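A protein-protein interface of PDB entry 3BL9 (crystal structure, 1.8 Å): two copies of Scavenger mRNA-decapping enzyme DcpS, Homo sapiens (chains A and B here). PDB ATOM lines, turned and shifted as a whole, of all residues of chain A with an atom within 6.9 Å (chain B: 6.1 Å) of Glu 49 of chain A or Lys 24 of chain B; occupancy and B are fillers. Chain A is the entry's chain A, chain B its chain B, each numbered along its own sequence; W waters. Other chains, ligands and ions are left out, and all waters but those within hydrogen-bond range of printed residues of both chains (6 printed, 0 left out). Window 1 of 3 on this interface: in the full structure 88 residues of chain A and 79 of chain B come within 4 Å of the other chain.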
ATOM      1  N   ARG A  22      -0.889 -24.638  13.427  1.00  0.00           N
ATOM      2  CA  ARG A  22      -0.202 -24.939  12.171  1.00  0.00           C
ATOM      3  C   ARG A  22       1.225 -24.419  12.161  1.00  0.00           C
ATOM      4  O   ARG A  22       2.141 -25.150  11.774  1.00  0.00           O
ATOM      5  CB  ARG A  22      -0.911 -24.364  10.942  1.00  0.00           C
ATOM      6  CG  ARG A  22      -0.163 -24.758   9.627  1.00  0.00           C
ATOM      7  CD  ARG A  22      -0.559 -23.942   8.408  1.00  0.00           C
ATOM      8  NE  ARG A  22      -0.067 -22.577   8.490  1.00  0.00           N
ATOM      9  CZ  ARG A  22      -0.326 -21.631   7.600  1.00  0.00           C
ATOM     10  NH1 ARG A  22      -1.068 -21.905   6.525  1.00  0.00           N
ATOM     11  NH2 ARG A  22       0.170 -20.407   7.787  1.00  0.00           N
ATOM     12  N   ASP A  23       1.390 -23.148  12.554  1.00  0.00           N
ATOM     13  CA  ASP A  23       2.692 -22.496  12.536  1.00  0.00           C
ATOM     14  C   ASP A  23       3.502 -22.737  13.834  1.00  0.00           C
ATOM     15  O   ASP A  23       4.719 -22.452  13.892  1.00  0.00           O
ATOM     16  CB  ASP A  23       2.510 -20.991  12.317  1.00  0.00           C
ATOM     17  CG  ASP A  23       2.139 -20.634  10.877  1.00  0.00           C
ATOM     18  OD1 ASP A  23       1.986 -21.511  10.001  1.00  0.00           O
ATOM     19  OD2 ASP A  23       2.015 -19.434  10.618  1.00  0.00           O
ATOM     20  N   LYS A  24       2.844 -23.261  14.867  1.00  0.00           N
ATOM     21  CA  LYS A  24       3.500 -23.496  16.183  1.00  0.00           C
ATOM     22  C   LYS A  24       4.078 -22.182  16.714  1.00  0.00           C
ATOM     23  O   LYS A  24       5.267 -22.058  17.017  1.00  0.00           O
ATOM     24  CB  LYS A  24       4.564 -24.608  16.128  1.00  0.00           C
ATOM     25  CG  LYS A  24       3.973 -26.016  15.924  1.00  0.00           C
ATOM     26  CD  LYS A  24       3.664 -26.251  14.483  1.00  0.00           C
ATOM     27  CE  LYS A  24       3.130 -27.639  14.191  1.00  0.00           C
ATOM     28  NZ  LYS A  24       2.621 -27.708  12.804  1.00  0.00           N
ATOM     29  N   ILE A  25       3.187 -21.204  16.834  1.00  0.00           N
ATOM     30  CA  ILE A  25       3.546 -19.900  17.292  1.00  0.00           C
ATOM     31  C   ILE A  25       2.486 -19.375  18.250  1.00  0.00           C
ATOM     32  O   ILE A  25       1.290 -19.730  18.165  1.00  0.00           O
ATOM     33  CB  ILE A  25       3.761 -18.948  16.077  1.00  0.00           C
ATOM     34  CG1 ILE A  25       4.320 -17.599  16.514  1.00  0.00           C
ATOM     35  CG2 ILE A  25       2.478 -18.751  15.317  1.00  0.00           C
ATOM     36  CD1 ILE A  25       4.918 -16.781  15.340  1.00  0.00           C
ATOM     37  N   ILE A  26       2.932 -18.545  19.178  1.00  0.00           N
ATOM     38  CA  ILE A  26       2.039 -17.881  20.111  1.00  0.00           C
ATOM     39  C   ILE A  26       2.509 -16.451  20.388  1.00  0.00           C
ATOM     40  O   ILE A  26       3.713 -16.209  20.498  1.00  0.00           O
ATOM     41  CB  ILE A  26       1.908 -18.716  21.415  1.00  0.00           C
ATOM     42  CG1 ILE A  26       0.780 -18.183  22.306  1.00  0.00           C
ATOM     43  CG2 ILE A  26       3.254 -18.797  22.183  1.00  0.00           C
ATOM     44  CD1 ILE A  26       0.280 -19.216  23.356  1.00  0.00           C
ATOM     45  N   ILE A  47       6.660 -13.177  21.687  1.00  0.00           N
ATOM     46  CA  ILE A  47       6.282 -14.075  20.614  1.00  0.00           C
ATOM     47  C   ILE A  47       7.216 -15.289  20.671  1.00  0.00           C
ATOM     48  O   ILE A  47       8.435 -15.127  20.682  1.00  0.00           O
ATOM     49  CB  ILE A  47       6.370 -13.392  19.221  1.00  0.00           C
ATOM     50  CG1 ILE A  47       5.607 -12.061  19.201  1.00  0.00           C
ATOM     51  CG2 ILE A  47       5.825 -14.338  18.136  1.00  0.00           C
ATOM     52  CD1 ILE A  47       5.957 -11.193  18.029  1.00  0.00           C
ATOM     53  N   LEU A  48       6.645 -16.490  20.746  1.00  0.00           N
ATOM     54  CA  LEU A  48       7.421 -17.733  20.790  1.00  0.00           C
ATOM     55  C   LEU A  48       7.087 -18.591  19.593  1.00  0.00           C
ATOM     56  O   LEU A  48       5.905 -18.824  19.315  1.00  0.00           O
ATOM     57  CB  LEU A  48       7.116 -18.519  22.058  1.00  0.00           C
ATOM     58  CG  LEU A  48       7.773 -17.992  23.334  1.00  0.00           C
ATOM     59  CD1 LEU A  48       6.920 -16.889  23.912  1.00  0.00           C
ATOM     60  CD2 LEU A  48       7.900 -19.134  24.312  1.00  0.00           C
ATOM     61  N   GLU A  49       8.118 -19.028  18.864  1.00  0.00           N
ATOM     62  CA  GLU A  49       7.936 -19.838  17.681  1.00  0.00           C
ATOM     63  C   GLU A  49       8.832 -21.087  17.740  1.00  0.00           C
ATOM     64  O   GLU A  49      10.028 -20.982  17.980  1.00  0.00           O
ATOM     65  CB  GLU A  49       8.269 -19.021  16.419  1.00  0.00           C
ATOM     66  CG  GLU A  49       7.802 -19.704  15.145  1.00  0.00           C
ATOM     67  CD  GLU A  49       8.073 -18.923  13.855  1.00  0.00           C
ATOM     68  OE1 GLU A  49       8.546 -17.766  13.915  1.00  0.00           O
ATOM     69  OE2 GLU A  49       7.800 -19.495  12.789  1.00  0.00           O
ATOM     70  N   LYS A  50       8.261 -22.264  17.527  1.00  0.00           N
ATOM     71  CA  LYS A  50       9.081 -23.460  17.399  1.00  0.00           C
ATOM     72  C   LYS A  50       9.929 -23.275  16.153  1.00  0.00           C
ATOM     73  O   LYS A  50       9.527 -22.594  15.202  1.00  0.00           O
ATOM     74  CB  LYS A  50       8.263 -24.743  17.333  1.00  0.00           C
ATOM     75  CG  LYS A  50       7.496 -25.056  18.601  1.00  0.00           C
ATOM     76  CD  LYS A  50       8.376 -25.488  19.724  1.00  0.00           C
ATOM     77  CE  LYS A  50       7.572 -25.781  20.999  1.00  0.00           C
ATOM     78  NZ  LYS A  50       6.671 -27.026  20.976  1.00  0.00           N
ATOM     79  N   THR A  51      11.121 -23.836  16.180  1.00  0.00           N
ATOM     80  CA  THR A  51      12.061 -23.652  15.097  1.00  0.00           C
ATOM     81  C   THR A  51      12.016 -24.794  14.078  1.00  0.00           C
ATOM     82  O   THR A  51      11.515 -25.899  14.379  1.00  0.00           O
ATOM     83  CB  THR A  51      13.493 -23.516  15.637  1.00  0.00           C
ATOM     84  OG1 THR A  51      13.809 -24.667  16.451  1.00  0.00           O
ATOM     85  CG2 THR A  51      13.651 -22.253  16.449  1.00  0.00           C
ATOM     86  N   PRO A  52      12.528 -24.541  12.865  1.00  0.00           N
ATOM     87  CA  PRO A  52      12.618 -25.609  11.875  1.00  0.00           C
ATOM     88  C   PRO A  52      13.583 -26.703  12.328  1.00  0.00           C
ATOM     89  O   PRO A  52      14.493 -26.462  13.163  1.00  0.00           O
ATOM     90  CB  PRO A  52      13.108 -24.893  10.599  1.00  0.00           C
ATOM     91  CG  PRO A  52      12.740 -23.408  10.840  1.00  0.00           C
ATOM     92  CD  PRO A  52      12.974 -23.240  12.311  1.00  0.00           C
ATOM     93  N   PHE A  53      13.356 -27.894  11.798  1.00  0.00           N
ATOM     94  CA  PHE A  53      14.195 -29.035  12.093  1.00  0.00           C
ATOM     95  C   PHE A  53      15.617 -28.921  11.547  1.00  0.00           C
ATOM     96  O   PHE A  53      15.869 -28.351  10.474  1.00  0.00           O
ATOM     97  CB  PHE A  53      13.540 -30.322  11.585  1.00  0.00           C
ATOM     98  CG  PHE A  53      12.419 -30.797  12.459  1.00  0.00           C
ATOM     99  CD1 PHE A  53      11.105 -30.465  12.168  1.00  0.00           C
ATOM    100  CD2 PHE A  53      12.686 -31.523  13.616  1.00  0.00           C
ATOM    101  CE1 PHE A  53      10.068 -30.881  12.982  1.00  0.00           C
ATOM    102  CE2 PHE A  53      11.635 -31.957  14.443  1.00  0.00           C
ATOM    103  CZ  PHE A  53      10.339 -31.623  14.127  1.00  0.00           C
ATOM    104  N   ASP A  90      15.467 -25.427  20.555  1.00  0.00           N
ATOM    105  CA  ASP A  90      15.459 -23.961  20.443  1.00  0.00           C
ATOM    106  C   ASP A  90      14.046 -23.451  20.082  1.00  0.00           C
ATOM    107  O   ASP A  90      13.410 -23.963  19.151  1.00  0.00           O
ATOM    108  CB  ASP A  90      16.470 -23.551  19.355  1.00  0.00           C
ATOM    109  CG  ASP A  90      16.623 -22.047  19.181  1.00  0.00           C
ATOM    110  OD1 ASP A  90      16.081 -21.233  19.970  1.00  0.00           O
ATOM    111  OD2 ASP A  90      17.346 -21.690  18.238  1.00  0.00           O
ATOM    112  N   VAL A  91      13.589 -22.439  20.820  1.00  0.00           N
ATOM    113  CA  VAL A  91      12.344 -21.721  20.532  1.00  0.00           C
ATOM    114  C   VAL A  91      12.736 -20.269  20.232  1.00  0.00           C
ATOM    115  O   VAL A  91      13.383 -19.617  21.048  1.00  0.00           O
ATOM    116  CB  VAL A  91      11.377 -21.773  21.724  1.00  0.00           C
ATOM    117  CG1 VAL A  91      10.223 -20.786  21.570  1.00  0.00           C
ATOM    118  CG2 VAL A  91      10.820 -23.210  21.880  1.00  0.00           C
ATOM    119  N   LYS A  92      12.401 -19.803  19.032  1.00  0.00           N
ATOM    120  CA  LYS A  92      12.691 -18.448  18.636  1.00  0.00           C
ATOM    121  C   LYS A  92      11.750 -17.496  19.399  1.00  0.00           C
ATOM    122  O   LYS A  92      10.530 -17.570  19.260  1.00  0.00           O
ATOM    123  CB  LYS A  92      12.509 -18.289  17.129  1.00  0.00           C
ATOM    124  CG  LYS A  92      12.869 -16.868  16.662  1.00  0.00           C
ATOM    125  CD  LYS A  92      13.430 -16.876  15.288  1.00  0.00           C
ATOM    126  CE  LYS A  92      13.912 -15.493  14.942  1.00  0.00           C
ATOM    127  NZ  LYS A  92      12.754 -14.559  14.931  1.00  0.00           N
ATOM    128  N   THR A  93      12.346 -16.607  20.182  1.00  0.00           N
ATOM    129  CA  THR A  93      11.617 -15.735  21.073  1.00  0.00           C
ATOM    130  C   THR A  93      11.843 -14.281  20.710  1.00  0.00           C
ATOM    131  O   THR A  93      12.984 -13.823  20.685  1.00  0.00           O
ATOM    132  CB  THR A  93      12.051 -16.039  22.509  1.00  0.00           C
ATOM    133  OG1 THR A  93      11.874 -17.444  22.733  1.00  0.00           O
ATOM    134  CG2 THR A  93      11.235 -15.254  23.515  1.00  0.00           C
ATOM    135  N   THR A  94      10.763 -13.560  20.429  1.00  0.00           N
ATOM    136  CA  THR A  94      10.857 -12.150  20.045  1.00  0.00           C
ATOM    137  C   THR A  94      10.085 -11.320  21.067  1.00  0.00           C
ATOM    138  O   THR A  94       8.930 -11.649  21.410  1.00  0.00           O
ATOM    139  CB  THR A  94      10.248 -11.933  18.676  1.00  0.00           C
ATOM    140  OG1 THR A  94      10.811 -12.880  17.771  1.00  0.00           O
ATOM    141  CG2 THR A  94      10.496 -10.478  18.155  1.00  0.00           C
ATOM    142  N   LYS A 171      12.632 -12.454  11.362  1.00  0.00           N
ATOM    143  CA  LYS A 171      11.967 -13.772  11.306  1.00  0.00           C
ATOM    144  C   LYS A 171      12.934 -14.948  11.240  1.00  0.00           C
ATOM    145  O   LYS A 171      12.609 -16.039  11.729  1.00  0.00           O
ATOM    146  CB  LYS A 171      11.005 -13.826  10.098  1.00  0.00           C
ATOM    147  CG  LYS A 171      10.259 -15.152   9.819  1.00  0.00           C
ATOM    148  CD  LYS A 171       9.184 -15.414  10.837  1.00  0.00           C
ATOM    149  CE  LYS A 171       8.273 -16.553  10.451  1.00  0.00           C
ATOM    150  NZ  LYS A 171       7.174 -16.603  11.461  1.00  0.00           N
ATOM    151  N   ASP A 179      14.528 -21.873   5.359  1.00  0.00           N
ATOM    152  CA  ASP A 179      13.711 -20.668   5.575  1.00  0.00           C
ATOM    153  C   ASP A 179      14.538 -19.385   5.394  1.00  0.00           C
ATOM    154  O   ASP A 179      14.250 -18.358   5.994  1.00  0.00           O
ATOM    155  CB  ASP A 179      12.997 -20.739   6.950  1.00  0.00           C
ATOM    156  CG  ASP A 179      13.954 -20.687   8.148  1.00  0.00           C
ATOM    157  OD1 ASP A 179      15.134 -21.079   8.018  1.00  0.00           O
ATOM    158  OD2 ASP A 179      13.507 -20.284   9.244  1.00  0.00           O
ATOM    159  N   PHE A 249      10.466 -22.171   1.035  1.00  0.00           N
ATOM    160  CA  PHE A 249       9.883 -21.611   2.243  1.00  0.00           C
ATOM    161  C   PHE A 249       8.575 -20.941   1.887  1.00  0.00           C
ATOM    162  O   PHE A 249       8.545 -20.061   1.020  1.00  0.00           O
ATOM    163  CB  PHE A 249      10.869 -20.593   2.823  1.00  0.00           C
ATOM    164  CG  PHE A 249      10.431 -19.914   4.111  1.00  0.00           C
ATOM    165  CD1 PHE A 249      10.920 -18.643   4.408  1.00  0.00           C
ATOM    166  CD2 PHE A 249       9.577 -20.523   5.041  1.00  0.00           C
ATOM    167  CE1 PHE A 249      10.557 -17.987   5.590  1.00  0.00           C
ATOM    168  CE2 PHE A 249       9.200 -19.849   6.220  1.00  0.00           C
ATOM    169  CZ  PHE A 249       9.696 -18.594   6.493  1.00  0.00           C
ATOM    170  N   SER B  20       8.648 -28.552   5.660  1.00  0.00           N
ATOM    171  CA  SER B  20       8.064 -27.222   5.734  1.00  0.00           C
ATOM    172  C   SER B  20       8.589 -26.495   6.978  1.00  0.00           C
ATOM    173  O   SER B  20       8.267 -26.871   8.119  1.00  0.00           O
ATOM    174  CB  SER B  20       6.541 -27.288   5.778  1.00  0.00           C
ATOM    175  OG  SER B  20       5.990 -26.007   6.077  1.00  0.00           O
ATOM    176  N   ALA B  21       9.367 -25.430   6.751  1.00  0.00           N
ATOM    177  CA  ALA B  21       9.808 -24.571   7.827  1.00  0.00           C
ATOM    178  C   ALA B  21       8.656 -23.751   8.374  1.00  0.00           C
ATOM    179  O   ALA B  21       8.642 -23.410   9.549  1.00  0.00           O
ATOM    180  CB  ALA B  21      10.989 -23.639   7.355  1.00  0.00           C
ATOM    181  N   ARG B  22       7.674 -23.422   7.539  1.00  0.00           N
ATOM    182  CA  ARG B  22       6.489 -22.739   8.048  1.00  0.00           C
ATOM    183  C   ARG B  22       5.720 -23.592   9.079  1.00  0.00           C
ATOM    184  O   ARG B  22       5.378 -23.110  10.160  1.00  0.00           O
ATOM    185  CB  ARG B  22       5.562 -22.328   6.895  1.00  0.00           C
ATOM    186  CG  ARG B  22       4.489 -21.348   7.348  1.00  0.00           C
ATOM    187  CD  ARG B  22       3.344 -21.250   6.364  1.00  0.00           C
ATOM    188  NE  ARG B  22       2.646 -22.536   6.199  1.00  0.00           N
ATOM    189  CZ  ARG B  22       1.922 -22.872   5.128  1.00  0.00           C
ATOM    190  NH1 ARG B  22       1.317 -24.049   5.084  1.00  0.00           N
ATOM    191  NH2 ARG B  22       1.751 -22.020   4.117  1.00  0.00           N
ATOM    192  N   ASP B  23       5.489 -24.854   8.750  1.00  0.00           N
ATOM    193  CA  ASP B  23       4.650 -25.719   9.578  1.00  0.00           C
ATOM    194  C   ASP B  23       5.449 -26.537  10.599  1.00  0.00           C
ATOM    195  O   ASP B  23       4.866 -27.342  11.339  1.00  0.00           O
ATOM    196  CB  ASP B  23       3.814 -26.664   8.709  1.00  0.00           C
ATOM    197  CG  ASP B  23       2.947 -25.940   7.691  1.00  0.00           C
ATOM    198  OD1 ASP B  23       2.755 -24.722   7.806  1.00  0.00           O
ATOM    199  OD2 ASP B  23       2.420 -26.619   6.784  1.00  0.00           O
ATOM    200  N   LYS B  24       6.765 -26.351  10.621  1.00  0.00           N
ATOM    201  CA  LYS B  24       7.657 -27.077  11.528  1.00  0.00           C
ATOM    202  C   LYS B  24       7.476 -28.606  11.429  1.00  0.00           C
ATOM    203  O   LYS B  24       7.265 -29.285  12.447  1.00  0.00           O
ATOM    204  CB  LYS B  24       7.457 -26.614  12.980  1.00  0.00           C
ATOM    205  CG  LYS B  24       7.171 -25.146  13.187  1.00  0.00           C
ATOM    206  CD  LYS B  24       8.265 -24.288  12.669  1.00  0.00           C
ATOM    207  CE  LYS B  24       7.972 -22.782  12.908  1.00  0.00           C
ATOM    208  NZ  LYS B  24       6.878 -22.098  12.189  1.00  0.00           N
ATOM    209  N   ILE B  25       7.577 -29.131  10.207  1.00  0.00           N
ATOM    210  CA  ILE B  25       7.376 -30.557   9.956  1.00  0.00           C
ATOM    211  C   ILE B  25       8.375 -31.050   8.918  1.00  0.00           C
ATOM    212  O   ILE B  25       8.746 -30.316   7.987  1.00  0.00           O
ATOM    213  CB  ILE B  25       5.932 -30.842   9.524  1.00  0.00           C
ATOM    214  CG1 ILE B  25       5.649 -32.347   9.460  1.00  0.00           C
ATOM    215  CG2 ILE B  25       5.602 -30.160   8.180  1.00  0.00           C
ATOM    216  CD1 ILE B  25       4.150 -32.656   9.373  1.00  0.00           C
ATOM    217  N   ILE B  26       8.831 -32.286   9.084  1.00  0.00           N
ATOM    218  CA  ILE B  26       9.745 -32.897   8.118  1.00  0.00           C
ATOM    219  C   ILE B  26       9.381 -34.384   7.931  1.00  0.00           C
ATOM    220  O   ILE B  26       8.930 -35.028   8.874  1.00  0.00           O
ATOM    221  CB  ILE B  26      11.212 -32.744   8.539  1.00  0.00           C
ATOM    222  CG1 ILE B  26      11.474 -33.295   9.938  1.00  0.00           C
ATOM    223  CG2 ILE B  26      11.627 -31.270   8.550  1.00  0.00           C
ATOM    224  CD1 ILE B  26      12.960 -33.489  10.235  1.00  0.00           C
ATOM    225  N   LEU B  48       8.368 -36.013  11.655  1.00  0.00           N
ATOM    226  CA  LEU B  48       8.521 -35.303  12.903  1.00  0.00           C
ATOM    227  C   LEU B  48       7.851 -33.940  12.781  1.00  0.00           C
ATOM    228  O   LEU B  48       8.007 -33.254  11.774  1.00  0.00           O
ATOM    229  CB  LEU B  48      10.003 -35.161  13.266  1.00  0.00           C
ATOM    230  CG  LEU B  48      10.828 -36.439  13.370  1.00  0.00           C
ATOM    231  CD1 LEU B  48      11.478 -36.800  12.043  1.00  0.00           C
ATOM    232  CD2 LEU B  48      11.900 -36.263  14.451  1.00  0.00           C
ATOM    233  N   GLU B  49       7.053 -33.592  13.774  1.00  0.00           N
ATOM    234  CA  GLU B  49       6.350 -32.326  13.786  1.00  0.00           C
ATOM    235  C   GLU B  49       6.505 -31.675  15.162  1.00  0.00           C
ATOM    236  O   GLU B  49       6.243 -32.297  16.186  1.00  0.00           O
ATOM    237  CB  GLU B  49       4.866 -32.528  13.440  1.00  0.00           C
ATOM    238  CG  GLU B  49       4.137 -31.225  13.098  1.00  0.00           C
ATOM    239  CD  GLU B  49       2.680 -31.418  12.721  1.00  0.00           C
ATOM    240  OE1 GLU B  49       1.995 -30.410  12.467  1.00  0.00           O
ATOM    241  OE2 GLU B  49       2.221 -32.573  12.677  1.00  0.00           O
ATOM    242  N   LYS B  50       6.908 -30.410  15.190  1.00  0.00           N
ATOM    243  CA  LYS B  50       6.985 -29.685  16.458  1.00  0.00           C
ATOM    244  C   LYS B  50       5.562 -29.498  16.975  1.00  0.00           C
ATOM    245  O   LYS B  50       4.586 -29.553  16.214  1.00  0.00           O
ATOM    246  CB  LYS B  50       7.726 -28.335  16.310  1.00  0.00           C
ATOM    247  CG  LYS B  50       9.105 -28.413  15.669  1.00  0.00           C
ATOM    248  CD  LYS B  50      10.199 -28.925  16.581  1.00  0.00           C
ATOM    249  CE  LYS B  50      11.628 -28.744  15.995  1.00  0.00           C
ATOM    250  NZ  LYS B  50      12.310 -27.472  16.386  1.00  0.00           N
ATOM    251  N   PHE B  53       2.307 -24.629  21.429  1.00  0.00           N
ATOM    252  CA  PHE B  53       2.531 -24.172  22.778  1.00  0.00           C
ATOM    253  C   PHE B  53       1.261 -24.302  23.588  1.00  0.00           C
ATOM    254  O   PHE B  53       0.159 -24.089  23.062  1.00  0.00           O
ATOM    255  CB  PHE B  53       2.951 -22.708  22.756  1.00  0.00           C
ATOM    256  CG  PHE B  53       4.308 -22.504  22.180  1.00  0.00           C
ATOM    257  CD1 PHE B  53       4.479 -22.076  20.881  1.00  0.00           C
ATOM    258  CD2 PHE B  53       5.430 -22.802  22.950  1.00  0.00           C
ATOM    259  CE1 PHE B  53       5.768 -21.921  20.349  1.00  0.00           C
ATOM    260  CE2 PHE B  53       6.724 -22.648  22.420  1.00  0.00           C
ATOM    261  CZ  PHE B  53       6.881 -22.217  21.126  1.00  0.00           C
HETATM  262  O   HOH W   1       8.900 -20.558   9.967  1.00  0.00           O
HETATM  263  O   HOH W   2       5.022 -20.167  10.570  1.00  0.00           O
HETATM  264  O   HOH W   3      11.082 -27.818   9.638  1.00  0.00           O
HETATM  265  O   HOH W   4      11.609 -26.007  18.516  1.00  0.00           O
HETATM  266  O   HOH W   5       1.159 -22.727  19.313  1.00  0.00           O
HETATM  267  O   HOH W   6      15.228 -28.067  15.988  1.00  0.00           O
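Water W4 lies within hydrogen-bond range of the side-chain amino group of Lys 50 of chain B, the backbone carbonyl oxygen of Asp 90 of chain A and the backbone NH of Thr 51 of chain A.
Water W1 lies within hydrogen-bond range of the backbone carbonyl oxygen of Ala 21 of chain B (2.9 Å), the side-chain carboxylate of Glu 49 of chain A (3.2 Å) and the side-chain amino group of Lys 24 of chain B (3.4 Å).
Water W2 lies within hydrogen-bond range of O of Arg 22 of chain B (3.0 Å), OD2 of Asp 23 of chain A (3.1 Å) and NZ of Lys 24 of chain B (3.1 Å).
Water W6 lies within hydrogen-bond range of NZ of Lys 50 of chain B and O of Pro 52 of chain A.
Water W5 lies within hydrogen-bond range of the backbone NH (N) of Phe 53 of chain B and the backbone carbonyl oxygen (O) of Ile 25 of chain A.
Water W3 lies within hydrogen-bond range of N of Phe 53 of chain A (3.1 Å) and O of Ser 20 of chain B (3.3 Å).
OD1 of Asp 23 of chain A is in salt-bridge range of NE of Arg 22 of chain A (2.8 Å).
NZ of Lys 24 of chain A sits at hydrogen-bond distance from O of Arg 22 of chain A (2.8 Å).
O of Lys 24 of chain A sits at hydrogen-bond distance from N of Lys 50 of chain A, 3.0 Å away.
The side-chain amino group (NZ) of Lys 171 of chain A is in salt-bridge range of the side-chain carboxylate (OE1) of Glu 49 of chain A, 3.0 Å away.
The side-chain hydroxyl (OG1) of Thr 51 of chain A lies within hydrogen-bond range of the backbone carbonyl oxygen (O) of Asp 90 of chain A, at 2.8 Å.
The guanidinium group (NE) of Arg 22 of chain B is in salt-bridge range of the side-chain carboxylate (OD1) of Asp 23 of chain B.
Along chain B the printed residues that touch a printed residue of chain A span positions 21 to 53.
Of the printed residues of chain B, Glu 49 of chain A touches Lys 24 (2.8 Å).
Of the printed residues of chain A, Lys 24 of chain B touches Asp 23, Lys 24, Glu 49, Lys 50 and Phe 53.
Of the printed residues of chain A, Phe 53 of chain B touches Lys 24 (3.4 Å), Ile 26 (3.7 Å), Leu 48 (3.3 Å), Lys 50 (3.5 Å) and Val 91 (3.7 Å).
Printed residues of chain B within 4 Å of Thr 51 of chain A: Lys 50 (2.7 Å).
Printed residues of chain A within 4 Å of Arg 22 of chain B: Arg 22 (3.4 Å) and Asp 23 (3.6 Å).
Of the printed residues of chain A, Glu 49 of chain B touches Lys 24 and Phe 53.
Of the printed residues of chain A, Lys 50 of chain B touches Lys 24 (3.1 Å), Lys 50 (3.8 Å), Thr 51 (2.7 Å) and Phe 53 (3.6 Å).
Ile 25 of chain B touches none of the printed residues of chain A.
The nearest printed residue of chain B that does not touch Glu 49 of chain A is Phe 53 of chain B (4.01 Å).
NE of Arg 22 of chain A is in salt-bridge range of OD1 of Asp 23 of chain B (3.6 Å).
OD1 of Asp 23 of chain A is in salt-bridge range of NE of Arg 22 of chain B (3.99 Å).
O of Asp 23 of chain A lies within hydrogen-bond range of NZ of Lys 24 of chain B, at 2.8 Å.
The backbone carbonyl oxygen (O) of Asp 23 of chain B is in hydrogen-bond range of the side-chain amino group (NZ) of Lys 24 of chain A, at 2.7 Å.
The side-chain amino group (NZ) of Lys 24 of chain A is in salt-bridge range of the side-chain carboxylate (OE1) of Glu 49 of chain B, 2.8 Å away.
NZ of Lys 24 of chain B is in salt-bridge range of OE2 of Glu 49 of chain A (2.8 Å).
The backbone carbonyl oxygen (O) of Thr 51 of chain A is in hydrogen-bond range of the side-chain amino group (NZ) of Lys 50 of chain B (2.7 Å).
Lys 24 of chain A touches Glu 49 of chain B, and with the chains exchanged Glu 49 of chain A touches Lys 24 of chain B.
Lys 24 of chain A touches Phe 53 of chain B, and with the chains exchanged Phe 53 of chain A touches Lys 24 of chain B.
Ile 26 of chain A touches Phe 53 of chain B, and with the chains exchanged Phe 53 of chain A touches Ile 26 of chain B.
Lys 50 of chain A touches Phe 53 of chain B, and with the chains exchanged Phe 53 of chain A touches Lys 50 of chain B.
Positions printed for both chains: 22, 23, 24, 25, 26, 48, 49, 50 and 53.
Lys 24 of chain B touches Lys 24 of chain A.
Phe 53 of chain B touches Lys 24 of chain A (CE1 to O, 3.4 Å).
Ile 26 of chain A touches Phe 53 of chain B (CG2 to CD1, 3.7 Å).
Lys 50 of chain A touches Lys 24 of chain B (O to CE, 2.8 Å).
Lys 50 of chain A touches Lys 50 of chain B.
Ala 21 of chain B touches Pro 52 of chain A (CB to CG, 3.9 Å).
Phe 53 of chain A touches Ile 26 of chain B (CB to CD1, 3.5 Å).
N of Glu 49 of chain B touches CZ of Phe 53 of chain A, at 3.8 Å.
Phe 53 of chain B touches Val 91 of chain A.
CB of Asp 179 of chain A touches CB of Ala 21 of chain B, 3.6 Å away.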
